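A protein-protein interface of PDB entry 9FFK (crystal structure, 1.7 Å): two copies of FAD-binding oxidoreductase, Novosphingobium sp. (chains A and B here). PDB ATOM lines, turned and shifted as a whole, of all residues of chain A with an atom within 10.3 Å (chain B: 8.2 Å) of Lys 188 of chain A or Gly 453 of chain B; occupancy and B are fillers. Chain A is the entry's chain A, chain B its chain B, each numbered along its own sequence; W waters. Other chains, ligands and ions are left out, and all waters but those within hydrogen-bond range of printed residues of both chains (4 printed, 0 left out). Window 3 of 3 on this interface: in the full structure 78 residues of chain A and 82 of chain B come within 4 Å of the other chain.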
ATOM      1  N   ARG A 181     -29.047  12.542 -28.189  1.00  0.00           N
ATOM      2  CA  ARG A 181     -30.340  12.155 -27.573  1.00  0.00           C
ATOM      3  C   ARG A 181     -30.388  12.772 -26.174  1.00  0.00           C
ATOM      4  O   ARG A 181     -29.442  12.620 -25.403  1.00  0.00           O
ATOM      5  CB  ARG A 181     -30.512  10.622 -27.584  1.00  0.00           C
ATOM      6  CG  ARG A 181     -30.494   9.977 -28.973  1.00  0.00           C
ATOM      7  CD  ARG A 181     -30.822   8.500 -28.868  1.00  0.00           C
ATOM      8  NE  ARG A 181     -31.166   8.005 -30.202  1.00  0.00           N
ATOM      9  CZ  ARG A 181     -31.655   6.804 -30.486  1.00  0.00           C
ATOM     10  NH1 ARG A 181     -31.919   5.918 -29.524  1.00  0.00           N
ATOM     11  NH2 ARG A 181     -31.919   6.522 -31.754  1.00  0.00           N
ATOM     12  N   THR A 182     -31.482  13.436 -25.835  1.00  0.00           N
ATOM     13  CA  THR A 182     -31.682  14.154 -24.573  1.00  0.00           C
ATOM     14  C   THR A 182     -32.161  13.167 -23.500  1.00  0.00           C
ATOM     15  O   THR A 182     -32.540  12.011 -23.846  1.00  0.00           O
ATOM     16  CB  THR A 182     -32.655  15.322 -24.743  1.00  0.00           C
ATOM     17  OG1 THR A 182     -33.954  14.796 -25.013  1.00  0.00           O
ATOM     18  CG2 THR A 182     -32.290  16.332 -25.818  1.00  0.00           C
ATOM     19  N   GLY A 183     -32.235  13.652 -22.263  1.00  0.00           N
ATOM     20  CA  GLY A 183     -32.783  12.930 -21.113  1.00  0.00           C
ATOM     21  C   GLY A 183     -31.952  11.656 -20.840  1.00  0.00           C
ATOM     22  O   GLY A 183     -30.694  11.658 -20.813  1.00  0.00           O
ATOM     23  N   MET A 184     -32.624  10.530 -20.896  1.00  0.00           N
ATOM     24  CA  MET A 184     -31.963   9.227 -20.645  1.00  0.00           C
ATOM     25  C   MET A 184     -31.538   8.573 -21.958  1.00  0.00           C
ATOM     26  O   MET A 184     -30.900   7.517 -21.893  1.00  0.00           O
ATOM     27  CB  MET A 184     -32.898   8.297 -19.879  1.00  0.00           C
ATOM     28  CG  MET A 184     -33.427   8.887 -18.597  1.00  0.00           C
ATOM     29  SD  MET A 184     -32.201   9.600 -17.511  1.00  0.00           S
ATOM     30  CE  MET A 184     -31.431   8.132 -16.849  1.00  0.00           C
ATOM     31  N   GLY A 185     -31.885   9.166 -23.111  1.00  0.00           N
ATOM     32  CA  GLY A 185     -31.699   8.621 -24.474  1.00  0.00           C
ATOM     33  C   GLY A 185     -30.264   8.277 -24.802  1.00  0.00           C
ATOM     34  O   GLY A 185     -30.038   7.355 -25.667  1.00  0.00           O
ATOM     35  N   SER A 186     -29.290   8.987 -24.233  1.00  0.00           N
ATOM     36  CA  SER A 186     -27.881   8.785 -24.644  1.00  0.00           C
ATOM     37  C   SER A 186     -27.225   7.631 -23.881  1.00  0.00           C
ATOM     38  O   SER A 186     -26.044   7.324 -24.221  1.00  0.00           O
ATOM     39  CB  SER A 186     -27.084  10.041 -24.528  1.00  0.00           C
ATOM     40  OG  SER A 186     -26.851  10.381 -23.166  1.00  0.00           O
ATOM     41  N   ILE A 187     -27.951   7.010 -22.963  1.00  0.00           N
ATOM     42  CA  ILE A 187     -27.513   5.778 -22.235  1.00  0.00           C
ATOM     43  C   ILE A 187     -27.828   4.573 -23.132  1.00  0.00           C
ATOM     44  O   ILE A 187     -28.986   4.290 -23.405  1.00  0.00           O
ATOM     45  CB  ILE A 187     -28.188   5.656 -20.857  1.00  0.00           C
ATOM     46  CG1 ILE A 187     -28.142   6.953 -20.043  1.00  0.00           C
ATOM     47  CG2 ILE A 187     -27.648   4.454 -20.079  1.00  0.00           C
ATOM     48  CD1 ILE A 187     -26.786   7.366 -19.635  1.00  0.00           C
ATOM     49  N   LYS A 188     -26.793   3.896 -23.598  1.00  0.00           N
ATOM     50  CA  LYS A 188     -26.897   2.643 -24.401  1.00  0.00           C
ATOM     51  C   LYS A 188     -27.812   1.682 -23.635  1.00  0.00           C
ATOM     52  O   LYS A 188     -27.540   1.404 -22.457  1.00  0.00           O
ATOM     53  CB  LYS A 188     -25.509   2.024 -24.637  1.00  0.00           C
ATOM     54  CG  LYS A 188     -24.343   3.005 -24.532  1.00  0.00           C
ATOM     55  CD  LYS A 188     -22.983   2.384 -24.795  1.00  0.00           C
ATOM     56  CE  LYS A 188     -21.857   3.387 -24.629  1.00  0.00           C
ATOM     57  NZ  LYS A 188     -20.630   2.947 -25.333  1.00  0.00           N
ATOM     58  N   GLY A 189     -28.876   1.243 -24.259  1.00  0.00           N
ATOM     59  CA  GLY A 189     -29.758   0.208 -23.686  1.00  0.00           C
ATOM     60  C   GLY A 189     -30.714   0.776 -22.666  1.00  0.00           C
ATOM     61  O   GLY A 189     -31.283   0.005 -21.915  1.00  0.00           O
ATOM     62  N   SER A 190     -30.909   2.101 -22.659  1.00  0.00           N
ATOM     63  CA  SER A 190     -31.919   2.757 -21.799  1.00  0.00           C
ATOM     64  C   SER A 190     -33.349   2.397 -22.227  1.00  0.00           C
ATOM     65  O   SER A 190     -33.702   2.540 -23.360  1.00  0.00           O
ATOM     66  CB  SER A 190     -31.734   4.251 -21.775  1.00  0.00           C
ATOM     67  OG  SER A 190     -32.702   4.801 -20.920  1.00  0.00           O
ATOM     68  N   THR A 191     -34.178   2.051 -21.270  1.00  0.00           N
ATOM     69  CA  THR A 191     -35.613   1.804 -21.463  1.00  0.00           C
ATOM     70  C   THR A 191     -36.394   2.937 -20.791  1.00  0.00           C
ATOM     71  O   THR A 191     -37.590   2.769 -20.560  1.00  0.00           O
ATOM     72  CB  THR A 191     -35.929   0.391 -20.938  1.00  0.00           C
ATOM     73  OG1 THR A 191     -35.719   0.422 -19.533  1.00  0.00           O
ATOM     74  CG2 THR A 191     -35.105  -0.704 -21.584  1.00  0.00           C
ATOM     75  N   ALA A 192     -35.765   4.075 -20.487  1.00  0.00           N
ATOM     76  CA  ALA A 192     -36.386   5.170 -19.702  1.00  0.00           C
ATOM     77  C   ALA A 192     -36.435   6.497 -20.495  1.00  0.00           C
ATOM     78  O   ALA A 192     -36.759   7.579 -19.908  1.00  0.00           O
ATOM     79  CB  ALA A 192     -35.628   5.283 -18.422  1.00  0.00           C
ATOM     80  N   TRP A 193     -36.191   6.416 -21.801  1.00  0.00           N
ATOM     81  CA  TRP A 193     -36.145   7.628 -22.675  1.00  0.00           C
ATOM     82  C   TRP A 193     -37.477   8.360 -22.647  1.00  0.00           C
ATOM     83  O   TRP A 193     -37.466   9.529 -22.586  1.00  0.00           O
ATOM     84  CB  TRP A 193     -35.785   7.245 -24.097  1.00  0.00           C
ATOM     85  CG  TRP A 193     -35.276   8.399 -24.903  1.00  0.00           C
ATOM     86  CD1 TRP A 193     -34.798   9.602 -24.450  1.00  0.00           C
ATOM     87  CD2 TRP A 193     -35.066   8.382 -26.325  1.00  0.00           C
ATOM     88  NE1 TRP A 193     -34.297  10.338 -25.499  1.00  0.00           N
ATOM     89  CE2 TRP A 193     -34.483   9.623 -26.655  1.00  0.00           C
ATOM     90  CE3 TRP A 193     -35.312   7.441 -27.345  1.00  0.00           C
ATOM     91  CZ2 TRP A 193     -34.100   9.894 -27.975  1.00  0.00           C
ATOM     92  CZ3 TRP A 193     -35.011   7.751 -28.658  1.00  0.00           C
ATOM     93  CH2 TRP A 193     -34.398   8.972 -28.944  1.00  0.00           C
ATOM     94  N   PHE A 196     -38.471   9.506 -18.109  1.00  0.00           N
ATOM     95  CA  PHE A 196     -37.950  10.546 -17.207  1.00  0.00           C
ATOM     96  C   PHE A 196     -37.505  11.742 -18.031  1.00  0.00           C
ATOM     97  O   PHE A 196     -36.604  11.513 -18.816  1.00  0.00           O
ATOM     98  CB  PHE A 196     -36.814  10.008 -16.327  1.00  0.00           C
ATOM     99  CG  PHE A 196     -36.236  11.027 -15.381  1.00  0.00           C
ATOM    100  CD1 PHE A 196     -37.052  11.708 -14.493  1.00  0.00           C
ATOM    101  CD2 PHE A 196     -34.896  11.412 -15.457  1.00  0.00           C
ATOM    102  CE1 PHE A 196     -36.556  12.653 -13.607  1.00  0.00           C
ATOM    103  CE2 PHE A 196     -34.410  12.412 -14.621  1.00  0.00           C
ATOM    104  CZ  PHE A 196     -35.230  13.049 -13.702  1.00  0.00           C
ATOM    105  N   PRO B 381     -30.032   6.283  -9.322  1.00  0.00           N
ATOM    106  CA  PRO B 381     -30.400   5.911 -10.685  1.00  0.00           C
ATOM    107  C   PRO B 381     -31.900   6.002 -10.948  1.00  0.00           C
ATOM    108  O   PRO B 381     -32.746   5.770 -10.057  1.00  0.00           O
ATOM    109  CB  PRO B 381     -29.869   4.473 -10.846  1.00  0.00           C
ATOM    110  CG  PRO B 381     -29.918   3.902  -9.397  1.00  0.00           C
ATOM    111  CD  PRO B 381     -29.621   5.101  -8.526  1.00  0.00           C
ATOM    112  N   VAL B 382     -32.198   6.319 -12.193  1.00  0.00           N
ATOM    113  CA  VAL B 382     -33.578   6.390 -12.765  1.00  0.00           C
ATOM    114  C   VAL B 382     -33.983   5.004 -13.248  1.00  0.00           C
ATOM    115  O   VAL B 382     -33.160   4.226 -13.738  1.00  0.00           O
ATOM    116  CB  VAL B 382     -33.575   7.437 -13.907  1.00  0.00           C
ATOM    117  CG1 VAL B 382     -34.869   7.516 -14.679  1.00  0.00           C
ATOM    118  CG2 VAL B 382     -33.134   8.810 -13.410  1.00  0.00           C
ATOM    119  N   ALA B 383     -35.283   4.740 -13.205  1.00  0.00           N
ATOM    120  CA  ALA B 383     -35.920   3.565 -13.798  1.00  0.00           C
ATOM    121  C   ALA B 383     -37.250   4.003 -14.429  1.00  0.00           C
ATOM    122  O   ALA B 383     -37.901   4.868 -13.839  1.00  0.00           O
ATOM    123  CB  ALA B 383     -36.104   2.551 -12.685  1.00  0.00           C
ATOM    124  N   GLU B 389     -37.754  -3.650 -13.777  1.00  0.00           N
ATOM    125  CA  GLU B 389     -36.645  -2.667 -13.650  1.00  0.00           C
ATOM    126  C   GLU B 389     -36.298  -2.494 -12.163  1.00  0.00           C
ATOM    127  O   GLU B 389     -35.102  -2.563 -11.865  1.00  0.00           O
ATOM    128  CB  GLU B 389     -36.987  -1.341 -14.356  1.00  0.00           C
ATOM    129  CG  GLU B 389     -36.748  -1.407 -15.869  1.00  0.00           C
ATOM    130  CD  GLU B 389     -36.825  -0.122 -16.693  1.00  0.00           C
ATOM    131  OE1 GLU B 389     -36.241   0.933 -16.281  1.00  0.00           O
ATOM    132  OE2 GLU B 389     -37.414  -0.186 -17.798  1.00  0.00           O
ATOM    133  N   ARG B 392     -34.628  -5.715 -10.863  1.00  0.00           N
ATOM    134  CA  ARG B 392     -33.245  -5.906 -11.320  1.00  0.00           C
ATOM    135  C   ARG B 392     -32.334  -4.861 -10.634  1.00  0.00           C
ATOM    136  O   ARG B 392     -31.187  -5.201 -10.326  1.00  0.00           O
ATOM    137  CB  ARG B 392     -33.162  -5.862 -12.851  1.00  0.00           C
ATOM    138  CG  ARG B 392     -33.822  -7.030 -13.575  1.00  0.00           C
ATOM    139  CD  ARG B 392     -33.700  -6.890 -15.080  1.00  0.00           C
ATOM    140  NE  ARG B 392     -32.290  -6.846 -15.420  1.00  0.00           N
ATOM    141  CZ  ARG B 392     -31.688  -6.044 -16.319  1.00  0.00           C
ATOM    142  NH1 ARG B 392     -32.375  -5.204 -17.080  1.00  0.00           N
ATOM    143  NH2 ARG B 392     -30.368  -6.115 -16.459  1.00  0.00           N
ATOM    144  N   GLN B 393     -32.783  -3.615 -10.458  1.00  0.00           N
ATOM    145  CA  GLN B 393     -31.937  -2.548  -9.859  1.00  0.00           C
ATOM    146  C   GLN B 393     -31.669  -2.863  -8.379  1.00  0.00           C
ATOM    147  O   GLN B 393     -30.514  -2.710  -7.921  1.00  0.00           O
ATOM    148  CB  GLN B 393     -32.590  -1.169  -9.984  1.00  0.00           C
ATOM    149  CG  GLN B 393     -32.418  -0.554 -11.365  1.00  0.00           C
ATOM    150  CD  GLN B 393     -32.593   0.944 -11.398  1.00  0.00           C
ATOM    151  OE1 GLN B 393     -32.636   1.606 -10.372  1.00  0.00           O
ATOM    152  NE2 GLN B 393     -32.700   1.506 -12.601  1.00  0.00           N
ATOM    153  N   LEU B 396     -29.040  -5.842  -8.225  1.00  0.00           N
ATOM    154  CA  LEU B 396     -27.639  -5.443  -8.524  1.00  0.00           C
ATOM    155  C   LEU B 396     -27.089  -4.538  -7.415  1.00  0.00           C
ATOM    156  O   LEU B 396     -25.898  -4.683  -7.046  1.00  0.00           O
ATOM    157  CB  LEU B 396     -27.636  -4.697  -9.862  1.00  0.00           C
ATOM    158  CG  LEU B 396     -26.259  -4.257 -10.374  1.00  0.00           C
ATOM    159  CD1 LEU B 396     -25.287  -5.423 -10.496  1.00  0.00           C
ATOM    160  CD2 LEU B 396     -26.386  -3.583 -11.722  1.00  0.00           C
ATOM    161  N   VAL B 446     -22.006   3.032  -9.918  1.00  0.00           N
ATOM    162  CA  VAL B 446     -22.241   3.887 -11.121  1.00  0.00           C
ATOM    163  C   VAL B 446     -21.882   3.075 -12.385  1.00  0.00           C
ATOM    164  O   VAL B 446     -22.641   3.021 -13.388  1.00  0.00           O
ATOM    165  CB  VAL B 446     -21.443   5.187 -11.030  1.00  0.00           C
ATOM    166  CG1 VAL B 446     -21.562   5.981 -12.321  1.00  0.00           C
ATOM    167  CG2 VAL B 446     -21.818   6.032  -9.827  1.00  0.00           C
ATOM    168  N   THR B 447     -20.742   2.385 -12.356  1.00  0.00           N
ATOM    169  CA  THR B 447     -20.175   1.798 -13.596  1.00  0.00           C
ATOM    170  C   THR B 447     -21.011   0.591 -14.015  1.00  0.00           C
ATOM    171  O   THR B 447     -21.370   0.434 -15.226  1.00  0.00           O
ATOM    172  CB  THR B 447     -18.688   1.489 -13.378  1.00  0.00           C
ATOM    173  OG1 THR B 447     -18.653   0.549 -12.321  1.00  0.00           O
ATOM    174  CG2 THR B 447     -17.903   2.706 -12.964  1.00  0.00           C
ATOM    175  N   ARG B 448     -21.381  -0.231 -13.037  1.00  0.00           N
ATOM    176  CA  ARG B 448     -22.116  -1.476 -13.333  1.00  0.00           C
ATOM    177  C   ARG B 448     -23.577  -1.134 -13.643  1.00  0.00           C
ATOM    178  O   ARG B 448     -24.103  -1.723 -14.533  1.00  0.00           O
ATOM    179  CB  ARG B 448     -21.883  -2.506 -12.253  1.00  0.00           C
ATOM    180  CG  ARG B 448     -20.490  -3.107 -12.360  1.00  0.00           C
ATOM    181  CD  ARG B 448     -20.289  -4.234 -11.382  1.00  0.00           C
ATOM    182  NE  ARG B 448     -21.187  -5.358 -11.657  1.00  0.00           N
ATOM    183  CZ  ARG B 448     -21.480  -6.325 -10.786  1.00  0.00           C
ATOM    184  NH1 ARG B 448     -20.966  -6.305  -9.566  1.00  0.00           N
ATOM    185  NH2 ARG B 448     -22.309  -7.297 -11.120  1.00  0.00           N
ATOM    186  N   PHE B 449     -24.217  -0.174 -12.978  1.00  0.00           N
ATOM    187  CA  PHE B 449     -25.589   0.282 -13.369  1.00  0.00           C
ATOM    188  C   PHE B 449     -25.574   0.802 -14.814  1.00  0.00           C
ATOM    189  O   PHE B 449     -26.480   0.474 -15.590  1.00  0.00           O
ATOM    190  CB  PHE B 449     -26.168   1.343 -12.419  1.00  0.00           C
ATOM    191  CG  PHE B 449     -26.981   0.734 -11.305  1.00  0.00           C
ATOM    192  CD1 PHE B 449     -26.399  -0.149 -10.405  1.00  0.00           C
ATOM    193  CD2 PHE B 449     -28.302   1.053 -11.138  1.00  0.00           C
ATOM    194  CE1 PHE B 449     -27.143  -0.718  -9.374  1.00  0.00           C
ATOM    195  CE2 PHE B 449     -29.056   0.487 -10.112  1.00  0.00           C
ATOM    196  CZ  PHE B 449     -28.461  -0.384  -9.216  1.00  0.00           C
ATOM    197  N   GLY B 450     -24.542   1.555 -15.164  1.00  0.00           N
ATOM    198  CA  GLY B 450     -24.428   2.188 -16.492  1.00  0.00           C
ATOM    199  C   GLY B 450     -24.301   1.120 -17.553  1.00  0.00           C
ATOM    200  O   GLY B 450     -25.021   1.224 -18.567  1.00  0.00           O
ATOM    201  N   ALA B 451     -23.503   0.083 -17.297  1.00  0.00           N
ATOM    202  CA  ALA B 451     -23.424  -1.099 -18.192  1.00  0.00           C
ATOM    203  C   ALA B 451     -24.814  -1.724 -18.445  1.00  0.00           C
ATOM    204  O   ALA B 451     -24.955  -2.316 -19.500  1.00  0.00           O
ATOM    205  CB  ALA B 451     -22.347  -2.108 -17.736  1.00  0.00           C
ATOM    206  N   GLN B 452     -25.775  -1.689 -17.506  1.00  0.00           N
ATOM    207  CA  GLN B 452     -27.142  -2.224 -17.640  1.00  0.00           C
ATOM    208  C   GLN B 452     -28.115  -1.178 -18.235  1.00  0.00           C
ATOM    209  O   GLN B 452     -29.341  -1.476 -18.284  1.00  0.00           O
ATOM    210  CB  GLN B 452     -27.638  -2.657 -16.265  1.00  0.00           C
ATOM    211  CG  GLN B 452     -26.878  -3.826 -15.670  1.00  0.00           C
ATOM    212  CD  GLN B 452     -26.673  -4.978 -16.625  1.00  0.00           C
ATOM    213  OE1 GLN B 452     -27.597  -5.460 -17.273  1.00  0.00           O
ATOM    214  NE2 GLN B 452     -25.429  -5.411 -16.750  1.00  0.00           N
ATOM    215  N   GLY B 453     -27.632   0.023 -18.612  1.00  0.00           N
ATOM    216  CA  GLY B 453     -28.429   1.064 -19.247  1.00  0.00           C
ATOM    217  C   GLY B 453     -29.085   2.008 -18.244  1.00  0.00           C
ATOM    218  O   GLY B 453     -30.011   2.733 -18.672  1.00  0.00           O
ATOM    219  N   TRP B 454     -28.619   2.040 -16.970  1.00  0.00           N
ATOM    220  CA  TRP B 454     -29.159   2.862 -15.857  1.00  0.00           C
ATOM    221  C   TRP B 454     -28.156   3.915 -15.403  1.00  0.00           C
ATOM    222  O   TRP B 454     -27.001   3.597 -15.177  1.00  0.00           O
ATOM    223  CB  TRP B 454     -29.534   2.004 -14.651  1.00  0.00           C
ATOM    224  CG  TRP B 454     -30.519   0.931 -14.942  1.00  0.00           C
ATOM    225  CD1 TRP B 454     -31.674   1.028 -15.659  1.00  0.00           C
ATOM    226  CD2 TRP B 454     -30.425  -0.442 -14.496  1.00  0.00           C
ATOM    227  NE1 TRP B 454     -32.294  -0.194 -15.704  1.00  0.00           N
ATOM    228  CE2 TRP B 454     -31.548  -1.113 -15.012  1.00  0.00           C
ATOM    229  CE3 TRP B 454     -29.474  -1.178 -13.775  1.00  0.00           C
ATOM    230  CZ2 TRP B 454     -31.752  -2.478 -14.806  1.00  0.00           C
ATOM    231  CZ3 TRP B 454     -29.681  -2.523 -13.566  1.00  0.00           C
ATOM    232  CH2 TRP B 454     -30.805  -3.161 -14.080  1.00  0.00           C
ATOM    233  N   ALA B 455     -28.625   5.141 -15.206  1.00  0.00           N
ATOM    234  CA  ALA B 455     -27.787   6.223 -14.705  1.00  0.00           C
ATOM    235  C   ALA B 455     -28.616   7.205 -13.857  1.00  0.00           C
ATOM    236  O   ALA B 455     -29.851   7.114 -13.778  1.00  0.00           O
ATOM    237  CB  ALA B 455     -27.113   6.920 -15.851  1.00  0.00           C
ATOM    238  N   SER B 456     -27.902   8.082 -13.172  1.00  0.00           N
ATOM    239  CA  SER B 456     -28.349   8.947 -12.083  1.00  0.00           C
ATOM    240  C   SER B 456     -29.085  10.171 -12.605  1.00  0.00           C
ATOM    241  O   SER B 456     -28.718  10.710 -13.621  1.00  0.00           O
ATOM    242  CB  SER B 456     -27.194   9.347 -11.195  1.00  0.00           C
ATOM    243  OG  SER B 456     -26.565   8.211 -10.658  1.00  0.00           O
ATOM    244  N   GLN B 469     -19.979  10.405 -17.523  1.00  0.00           N
ATOM    245  CA  GLN B 469     -19.365   9.424 -18.475  1.00  0.00           C
ATOM    246  C   GLN B 469     -20.372   8.343 -18.853  1.00  0.00           C
ATOM    247  O   GLN B 469     -20.087   7.632 -19.828  1.00  0.00           O
ATOM    248  CB  GLN B 469     -18.126   8.804 -17.857  1.00  0.00           C
ATOM    249  CG  GLN B 469     -16.951   9.779 -17.886  1.00  0.00           C
ATOM    250  CD  GLN B 469     -15.797   9.408 -16.980  1.00  0.00           C
ATOM    251  OE1 GLN B 469     -15.541   8.228 -16.701  1.00  0.00           O
ATOM    252  NE2 GLN B 469     -15.077  10.429 -16.526  1.00  0.00           N
ATOM    253  N   GLN B 470     -21.431   8.124 -18.047  1.00  0.00           N
ATOM    254  CA  GLN B 470     -22.500   7.153 -18.353  1.00  0.00           C
ATOM    255  C   GLN B 470     -23.286   7.666 -19.540  1.00  0.00           C
ATOM    256  O   GLN B 470     -23.780   6.843 -20.272  1.00  0.00           O
ATOM    257  CB  GLN B 470     -23.405   6.859 -17.165  1.00  0.00           C
ATOM    258  CG  GLN B 470     -22.651   6.320 -15.949  1.00  0.00           C
ATOM    259  CD  GLN B 470     -21.520   5.363 -16.310  1.00  0.00           C
ATOM    260  OE1 GLN B 470     -21.759   4.327 -16.920  1.00  0.00           O
ATOM    261  NE2 GLN B 470     -20.284   5.709 -15.941  1.00  0.00           N
ATOM    262  N   TYR B 471     -23.415   8.986 -19.687  1.00  0.00           N
ATOM    263  CA  TYR B 471     -24.230   9.631 -20.753  1.00  0.00           C
ATOM    264  C   TYR B 471     -23.357   9.800 -21.997  1.00  0.00           C
ATOM    265  O   TYR B 471     -22.187   9.379 -21.954  1.00  0.00           O
ATOM    266  CB  TYR B 471     -24.822  10.964 -20.272  1.00  0.00           C
ATOM    267  CG  TYR B 471     -25.848  10.821 -19.200  1.00  0.00           C
ATOM    268  CD1 TYR B 471     -25.498  10.755 -17.856  1.00  0.00           C
ATOM    269  CD2 TYR B 471     -27.182  10.694 -19.528  1.00  0.00           C
ATOM    270  CE1 TYR B 471     -26.474  10.546 -16.887  1.00  0.00           C
ATOM    271  CE2 TYR B 471     -28.152  10.482 -18.577  1.00  0.00           C
ATOM    272  CZ  TYR B 471     -27.801  10.427 -17.238  1.00  0.00           C
ATOM    273  OH  TYR B 471     -28.786  10.208 -16.296  1.00  0.00           O
ATOM    274  N   GLY B 472     -23.944  10.309 -23.088  1.00  0.00           N
ATOM    275  CA  GLY B 472     -23.314  10.256 -24.411  1.00  0.00           C
ATOM    276  C   GLY B 472     -22.106  11.158 -24.481  1.00  0.00           C
ATOM    277  O   GLY B 472     -22.113  12.282 -23.851  1.00  0.00           O
ATOM    278  N   GLU B 473     -21.137  10.773 -25.305  1.00  0.00           N
ATOM    279  CA  GLU B 473     -19.988  11.647 -25.647  1.00  0.00           C
ATOM    280  C   GLU B 473     -20.482  12.916 -26.341  1.00  0.00           C
ATOM    281  O   GLU B 473     -19.900  14.007 -26.049  1.00  0.00           O
ATOM    282  CB  GLU B 473     -18.975  10.915 -26.524  1.00  0.00           C
ATOM    283  CG  GLU B 473     -17.814  11.798 -26.953  1.00  0.00           C
ATOM    284  CD  GLU B 473     -17.037  12.569 -25.881  1.00  0.00           C
ATOM    285  OE1 GLU B 473     -16.875  12.065 -24.742  1.00  0.00           O
ATOM    286  OE2 GLU B 473     -16.545  13.675 -26.200  1.00  0.00           O
ATOM    287  N   ARG B 476     -21.705  15.282 -23.626  1.00  0.00           N
ATOM    288  CA  ARG B 476     -20.527  15.853 -22.887  1.00  0.00           C
ATOM    289  C   ARG B 476     -19.940  16.969 -23.768  1.00  0.00           C
ATOM    290  O   ARG B 476     -19.696  18.077 -23.263  1.00  0.00           O
ATOM    291  CB  ARG B 476     -19.494  14.745 -22.612  1.00  0.00           C
ATOM    292  CG  ARG B 476     -18.851  14.685 -21.235  1.00  0.00           C
ATOM    293  CD  ARG B 476     -18.854  13.229 -20.743  1.00  0.00           C
ATOM    294  NE  ARG B 476     -18.123  12.242 -21.587  1.00  0.00           N
ATOM    295  CZ  ARG B 476     -18.604  11.087 -22.075  1.00  0.00           C
ATOM    296  NH1 ARG B 476     -19.827  10.660 -21.815  1.00  0.00           N
ATOM    297  NH2 ARG B 476     -17.843  10.334 -22.840  1.00  0.00           N
HETATM  298  O   HOH W   1     -31.811  -0.659 -19.189  1.00  0.00           O
HETATM  299  O   HOH W   2     -34.146   1.961 -17.582  1.00  0.00           O
HETATM  300  O   HOH W   3     -34.135  -1.490 -18.063  1.00  0.00           O
HETATM  301  O   HOH W   4     -31.749   4.571 -18.445  1.00  0.00           O
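The side-chain sulfur (SD) of Met 184 of chain A lies close to the side-chain hydroxyl (OH) of Tyr 471 of chain B (3.7 Å).
OG of Ser 186 of chain A lies within hydrogen-bond range of N of Gly 472 of chain B (2.9 Å).
OG1 of Thr 191 of chain A sits at hydrogen-bond distance from OE2 of Glu 389 of chain B, 2.5 Å away.
The backbone NH (N) of Ala 192 of chain A is in hydrogen-bond range of the side-chain hydroxyl (OG) of Ser 190 of chain A (3.2 Å).
O of Val 382 of chain B sits at hydrogen-bond distance from NE2 of Gln 393 of chain B.
The backbone carbonyl oxygen of Ala 455 of chain B lies within hydrogen-bond range of the backbone NH of Val 382 of chain B (2.9 Å).
The backbone carbonyl oxygen (O) of Tyr 471 of chain B lies within hydrogen-bond range of the guanidinium group (NH1) of Arg 476 of chain B, 2.7 Å away.
The backbone carbonyl oxygen (O) of Gly 472 of chain B sits at hydrogen-bond distance from the guanidinium group (NH1) of Arg 476 of chain B.
Gly 183 of chain A touches Tyr 471 of chain B.
Ala 455 of chain B touches Met 184 of chain A.
OG of Ser 186 of chain A touches CB of Tyr 471 of chain B, 3.6 Å away.
CG2 of Ile 187 of chain A touches O of Gly 453 of chain B, at 3.2 Å.
Ile 187 of chain A touches Ala 455 of chain B.
Gln 470 of chain B touches Ile 187 of chain A (O to CD1, 3.1 Å).
Ile 187 of chain A touches Tyr 471 of chain B (CD1 to CD2, 3.4 Å).
Lys 188 of chain A touches Gly 453 of chain B.
CA of Ser 190 of chain A touches O of Gly 453 of chain B (3.7 Å).
CG1 of Val 382 of chain B touches CB of Phe 196 of chain A (3.6 Å).
Of the printed residues of chain B, Met 184 of chain A touches Val 382 (3.7 Å), Ala 455 (3.6 Å) and Tyr 471 (3.4 Å).
Of chain B, only Gly 453 comes within 4 Å of Lys 188 of chain A.
No residue of chain B comes within 4 Å of Gly 189 of chain A.
Of the printed residues of chain B, Thr 191 of chain A touches Glu 389 (2.5 Å).
No residue of chain A comes within 4 Å of Gln 452 of chain B.
Of chain A, only Ile 187 (3.2 Å), Lys 188 (3.3 Å) and Ser 190 (3.7 Å) come within 4 Å of Gly 453 of chain B.
Of the printed residues of chain A, Ala 455 of chain B touches Met 184 and Ile 187.
Of the printed residues of chain A, Gly 472 of chain B touches Ser 186.
The nearest residue of chain A that does not touch Gly 453 of chain B is Gly 189 of chain A (4.05 Å).
Of the 14 printed residues of chain A, 8 touch a printed residue of chain B.
Printed residues of chain A that touch a printed residue of chain B: Gly 183, Met 184, Ser 186, Ile 187, Lys 188, Ser 190, Thr 191 and Phe 196.
Of the 24 printed residues of chain B, 7 touch a printed residue of chain A.
Hydrophobic or aromatic side chains of chain B that line the printed part of chain A: Val 382, Ala 455 and Tyr 471.
Along chain B the printed residues that touch a printed residue of chain A span positions 382 to 472.
No position is printed for both chains.
Of the 14 pairs that touch across the chains among the printed residues, none has its exchanged pair printed and touching as well.
Water W4 bridges the backbone carbonyl oxygen (O) of Gly 453 of chain B (2.5 Å) and the side-chain hydroxyl (OG) of Ser 190 of chain A (2.7 Å).
Water W2 lies within hydrogen-bond range of OE1 of Glu 389 of chain B (2.7 Å), OG1 of Thr 191 of chain A (2.9 Å) and NE1 of Trp 454 of chain B (3.4 Å).
Water W1 bridges the backbone carbonyl oxygen (O) of Gln 452 of chain B (2.8 Å) and the backbone carbonyl oxygen (O) of Gly 189 of chain A (2.9 Å).
Water W3 lies within hydrogen-bond range of the side-chain hydroxyl (OG1) of Thr 191 of chain A (2.9 Å) and the indole nitrogen (NE1) of Trp 454 of chain B (3.3 Å).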
